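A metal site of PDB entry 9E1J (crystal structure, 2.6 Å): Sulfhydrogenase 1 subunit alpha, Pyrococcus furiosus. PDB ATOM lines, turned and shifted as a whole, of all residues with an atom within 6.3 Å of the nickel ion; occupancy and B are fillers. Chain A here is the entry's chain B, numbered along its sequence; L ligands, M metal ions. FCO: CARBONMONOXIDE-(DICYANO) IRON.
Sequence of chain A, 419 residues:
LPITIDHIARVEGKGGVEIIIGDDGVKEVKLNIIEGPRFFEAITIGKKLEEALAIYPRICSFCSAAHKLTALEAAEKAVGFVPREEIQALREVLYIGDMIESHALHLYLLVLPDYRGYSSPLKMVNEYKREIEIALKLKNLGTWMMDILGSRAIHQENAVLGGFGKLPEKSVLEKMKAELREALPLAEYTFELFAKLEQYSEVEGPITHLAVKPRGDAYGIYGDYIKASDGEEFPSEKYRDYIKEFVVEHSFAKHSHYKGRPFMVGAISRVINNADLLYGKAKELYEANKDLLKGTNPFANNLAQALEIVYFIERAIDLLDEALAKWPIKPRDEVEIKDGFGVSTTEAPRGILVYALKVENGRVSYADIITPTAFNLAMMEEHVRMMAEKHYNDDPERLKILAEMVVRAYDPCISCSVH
SG of Cys 60 lies close to N of Phe 62.
OG1 of Thr 373 is in hydrogen-bond range of N of Cys 413 (3.1 Å).
The side-chain sulfur of Cys 413 sits close to the side-chain carboxylate of Glu 12, at 2.9 Å.
SG of Cys 416 lies close to NE2 of His 67, 3.5 Å away.
The backbone NH of Arg 350 lies within hydrogen-bond range of a nitrogen (N2) of the ligand, at 2.8 Å.
N of Thr 373 is in hydrogen-bond range of N1 of the ligand, at 2.9 Å.
The side-chain sulfur (SG) of Cys 63 binds an iron atom (FE) of the ligand, 2.5 Å away.
An iron atom (FE) of the ligand is bound by the side-chain sulfur (SG) of Cys 416.
The nickel ion is bound by the side-chain sulfur (SG) of Cys 416 (2.0 Å), the side-chain sulfur (SG) of Cys 413 (2.1 Å), the side-chain sulfur (SG) of Cys 60 (2.1 Å) and the side-chain sulfur (SG) of Cys 63 (2.2 Å).
Of the 16 residues printed, 4 come within 4 Å of the nickel ion.
Along chain A the residues within 4 Å of the nickel ion span positions 60 to 416.
The nearest printed residue that does not touch the nickel ion is Arg 350 (4.5 Å).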
ATOM      1  N   GLU A  12     -13.994  33.134  -7.940  1.00  0.00           N
ATOM      2  CA  GLU A  12     -15.207  32.784  -8.644  1.00  0.00           C
ATOM      3  C   GLU A  12     -16.424  33.354  -7.910  1.00  0.00           C
ATOM      4  O   GLU A  12     -16.542  33.212  -6.693  1.00  0.00           O
ATOM      5  CB  GLU A  12     -15.328  31.260  -8.733  1.00  0.00           C
ATOM      6  CG  GLU A  12     -16.262  30.796  -9.749  1.00  0.00           C
ATOM      7  CD  GLU A  12     -17.708  30.957  -9.296  1.00  0.00           C
ATOM      8  OE1 GLU A  12     -18.023  30.571  -8.150  1.00  0.00           O
ATOM      9  OE2 GLU A  12     -18.550  31.484 -10.073  1.00  0.00           O
ATOM     10  N   ILE A  59     -24.106  24.498 -11.061  1.00  0.00           N
ATOM     11  CA  ILE A  59     -23.824  25.208  -9.823  1.00  0.00           C
ATOM     12  C   ILE A  59     -22.485  25.904  -9.922  1.00  0.00           C
ATOM     13  O   ILE A  59     -22.293  26.990  -9.368  1.00  0.00           O
ATOM     14  CB  ILE A  59     -23.896  24.227  -8.625  1.00  0.00           C
ATOM     15  CG1 ILE A  59     -25.348  24.059  -8.175  1.00  0.00           C
ATOM     16  CG2 ILE A  59     -23.197  24.803  -7.469  1.00  0.00           C
ATOM     17  CD1 ILE A  59     -25.639  22.780  -7.321  1.00  0.00           C
ATOM     18  N   CYS A  60     -21.528  25.334 -10.651  1.00  0.00           N
ATOM     19  CA  CYS A  60     -20.175  25.858 -10.581  1.00  0.00           C
ATOM     20  C   CYS A  60     -19.350  25.337 -11.727  1.00  0.00           C
ATOM     21  O   CYS A  60     -19.407  24.148 -12.034  1.00  0.00           O
ATOM     22  CB  CYS A  60     -19.498  25.446  -9.267  1.00  0.00           C
ATOM     23  SG  CYS A  60     -17.869  26.144  -9.080  1.00  0.00           S
ATOM     24  N   SER A  61     -18.552  26.226 -12.336  1.00  0.00           N
ATOM     25  CA  SER A  61     -17.761  25.815 -13.499  1.00  0.00           C
ATOM     26  C   SER A  61     -16.385  25.277 -13.128  1.00  0.00           C
ATOM     27  O   SER A  61     -15.877  24.373 -13.804  1.00  0.00           O
ATOM     28  CB  SER A  61     -17.542  26.983 -14.426  1.00  0.00           C
ATOM     29  OG  SER A  61     -17.088  28.049 -13.637  1.00  0.00           O
ATOM     30  N   PHE A  62     -15.792  25.797 -12.079  1.00  0.00           N
ATOM     31  CA  PHE A  62     -14.497  25.290 -11.640  1.00  0.00           C
ATOM     32  C   PHE A  62     -14.589  23.883 -11.090  1.00  0.00           C
ATOM     33  O   PHE A  62     -13.611  23.131 -11.202  1.00  0.00           O
ATOM     34  CB  PHE A  62     -13.900  26.225 -10.591  1.00  0.00           C
ATOM     35  CG  PHE A  62     -13.542  27.574 -11.100  1.00  0.00           C
ATOM     36  CD1 PHE A  62     -14.489  28.370 -11.720  1.00  0.00           C
ATOM     37  CD2 PHE A  62     -12.261  28.039 -10.985  1.00  0.00           C
ATOM     38  CE1 PHE A  62     -14.163  29.609 -12.194  1.00  0.00           C
ATOM     39  CE2 PHE A  62     -11.940  29.286 -11.462  1.00  0.00           C
ATOM     40  CZ  PHE A  62     -12.906  30.070 -12.078  1.00  0.00           C
ATOM     41  N   CYS A  63     -15.705  23.525 -10.457  1.00  0.00           N
ATOM     42  CA  CYS A  63     -15.887  22.207  -9.834  1.00  0.00           C
ATOM     43  C   CYS A  63     -17.003  21.400 -10.494  1.00  0.00           C
ATOM     44  O   CYS A  63     -17.408  20.350  -9.964  1.00  0.00           O
ATOM     45  CB  CYS A  63     -16.189  22.372  -8.332  1.00  0.00           C
ATOM     46  SG  CYS A  63     -17.217  23.778  -8.030  1.00  0.00           S
ATOM     47  N   SER A  64     -17.491  21.859 -11.634  1.00  0.00           N
ATOM     48  CA  SER A  64     -18.498  21.199 -12.452  1.00  0.00           C
ATOM     49  C   SER A  64     -18.488  19.677 -12.347  1.00  0.00           C
ATOM     50  O   SER A  64     -19.496  19.052 -12.027  1.00  0.00           O
ATOM     51  CB  SER A  64     -18.268  21.595 -13.885  1.00  0.00           C
ATOM     52  OG  SER A  64     -19.502  21.695 -14.550  1.00  0.00           O
ATOM     53  N   HIS A  67     -19.451  18.204  -9.029  1.00  0.00           N
ATOM     54  CA  HIS A  67     -20.886  18.190  -8.751  1.00  0.00           C
ATOM     55  C   HIS A  67     -21.532  16.976  -9.406  1.00  0.00           C
ATOM     56  O   HIS A  67     -22.022  16.083  -8.721  1.00  0.00           O
ATOM     57  CB  HIS A  67     -21.529  19.514  -9.186  1.00  0.00           C
ATOM     58  CG  HIS A  67     -21.305  20.618  -8.188  1.00  0.00           C
ATOM     59  ND1 HIS A  67     -22.185  20.873  -7.165  1.00  0.00           N
ATOM     60  CD2 HIS A  67     -20.280  21.489  -8.022  1.00  0.00           C
ATOM     61  CE1 HIS A  67     -21.722  21.867  -6.423  1.00  0.00           C
ATOM     62  NE2 HIS A  67     -20.565  22.256  -6.929  1.00  0.00           N
ATOM     63  N   ARG A 350     -11.957  22.215  -3.422  1.00  0.00           N
ATOM     64  CA  ARG A 350     -12.009  23.193  -2.354  1.00  0.00           C
ATOM     65  C   ARG A 350     -12.324  22.604  -0.988  1.00  0.00           C
ATOM     66  O   ARG A 350     -12.184  23.303   0.016  1.00  0.00           O
ATOM     67  CB  ARG A 350     -13.025  24.252  -2.754  1.00  0.00           C
ATOM     68  CG  ARG A 350     -12.346  25.136  -3.776  1.00  0.00           C
ATOM     69  CD  ARG A 350     -13.256  25.737  -4.760  1.00  0.00           C
ATOM     70  NE  ARG A 350     -12.515  26.445  -5.801  1.00  0.00           N
ATOM     71  CZ  ARG A 350     -12.105  25.938  -6.967  1.00  0.00           C
ATOM     72  NH1 ARG A 350     -12.262  24.668  -7.278  1.00  0.00           N
ATOM     73  NH2 ARG A 350     -11.533  26.760  -7.849  1.00  0.00           N
ATOM     74  N   THR A 373     -16.861  25.656  -0.038  1.00  0.00           N
ATOM     75  CA  THR A 373     -16.732  27.059   0.277  1.00  0.00           C
ATOM     76  C   THR A 373     -17.804  27.486   1.266  1.00  0.00           C
ATOM     77  O   THR A 373     -17.558  28.352   2.102  1.00  0.00           O
ATOM     78  CB  THR A 373     -16.733  27.867  -1.031  1.00  0.00           C
ATOM     79  OG1 THR A 373     -15.470  27.651  -1.657  1.00  0.00           O
ATOM     80  CG2 THR A 373     -16.804  29.346  -0.799  1.00  0.00           C
ATOM     81  N   PRO A 412     -12.008  30.338  -2.832  1.00  0.00           N
ATOM     82  CA  PRO A 412     -13.466  30.390  -2.763  1.00  0.00           C
ATOM     83  C   PRO A 412     -14.112  30.267  -4.132  1.00  0.00           C
ATOM     84  O   PRO A 412     -13.825  31.030  -5.061  1.00  0.00           O
ATOM     85  CB  PRO A 412     -13.734  31.753  -2.135  1.00  0.00           C
ATOM     86  CG  PRO A 412     -12.549  32.540  -2.476  1.00  0.00           C
ATOM     87  CD  PRO A 412     -11.393  31.655  -2.712  1.00  0.00           C
ATOM     88  N   CYS A 413     -15.011  29.340  -4.268  1.00  0.00           N
ATOM     89  CA  CYS A 413     -15.956  29.405  -5.363  1.00  0.00           C
ATOM     90  C   CYS A 413     -17.295  29.747  -4.732  1.00  0.00           C
ATOM     91  O   CYS A 413     -17.943  28.903  -4.106  1.00  0.00           O
ATOM     92  CB  CYS A 413     -15.944  28.111  -6.171  1.00  0.00           C
ATOM     93  SG  CYS A 413     -17.266  27.861  -7.337  1.00  0.00           S
ATOM     94  N   ILE A 414     -17.665  31.017  -4.865  1.00  0.00           N
ATOM     95  CA  ILE A 414     -18.848  31.537  -4.203  1.00  0.00           C
ATOM     96  C   ILE A 414     -20.104  30.934  -4.828  1.00  0.00           C
ATOM     97  O   ILE A 414     -21.062  30.583  -4.120  1.00  0.00           O
ATOM     98  CB  ILE A 414     -18.817  33.063  -4.304  1.00  0.00           C
ATOM     99  CG1 ILE A 414     -17.765  33.594  -3.322  1.00  0.00           C
ATOM    100  CG2 ILE A 414     -20.209  33.653  -4.062  1.00  0.00           C
ATOM    101  CD1 ILE A 414     -17.797  35.052  -3.120  1.00  0.00           C
ATOM    102  N   SER A 415     -20.128  30.804  -6.162  1.00  0.00           N
ATOM    103  CA  SER A 415     -21.211  30.132  -6.860  1.00  0.00           C
ATOM    104  C   SER A 415     -21.508  28.781  -6.252  1.00  0.00           C
ATOM    105  O   SER A 415     -22.657  28.391  -6.145  1.00  0.00           O
ATOM    106  CB  SER A 415     -20.881  29.976  -8.355  1.00  0.00           C
ATOM    107  OG  SER A 415     -20.833  31.198  -9.072  1.00  0.00           O
ATOM    108  N   CYS A 416     -20.486  28.008  -5.873  1.00  0.00           N
ATOM    109  CA  CYS A 416     -20.759  26.774  -5.146  1.00  0.00           C
ATOM    110  C   CYS A 416     -21.471  27.075  -3.835  1.00  0.00           C
ATOM    111  O   CYS A 416     -22.372  26.335  -3.401  1.00  0.00           O
ATOM    112  CB  CYS A 416     -19.459  26.041  -4.832  1.00  0.00           C
ATOM    113  SG  CYS A 416     -18.715  25.128  -6.173  1.00  0.00           S
ATOM    114  N   SER A 417     -21.108  28.194  -3.191  1.00  0.00           N
ATOM    115  CA  SER A 417     -21.597  28.446  -1.837  1.00  0.00           C
ATOM    116  C   SER A 417     -23.088  28.753  -1.840  1.00  0.00           C
ATOM    117  O   SER A 417     -23.829  28.192  -1.034  1.00  0.00           O
ATOM    118  CB  SER A 417     -20.771  29.566  -1.191  1.00  0.00           C
ATOM    119  OG  SER A 417     -21.146  30.808  -1.738  1.00  0.00           O
HETATM  120 FE   FCO L   1     -17.119  23.762  -5.578  1.00  0.00          FE
HETATM  121  C1  FCO L   1     -17.343  24.536  -3.866  1.00  0.00           C
HETATM  122  N1  FCO L   1     -17.453  25.007  -2.816  1.00  0.00           N
HETATM  123  C2  FCO L   1     -15.327  23.173  -5.190  1.00  0.00           C
HETATM  124  N2  FCO L   1     -14.264  22.731  -4.991  1.00  0.00           N
HETATM  125  C3  FCO L   1     -17.593  22.204  -5.009  1.00  0.00           C
HETATM  126  O3  FCO L   1     -17.911  21.130  -4.695  1.00  0.00           O
HETATM  127 NI    NI M   1     -17.042  25.774  -7.147  1.00  0.00          NI
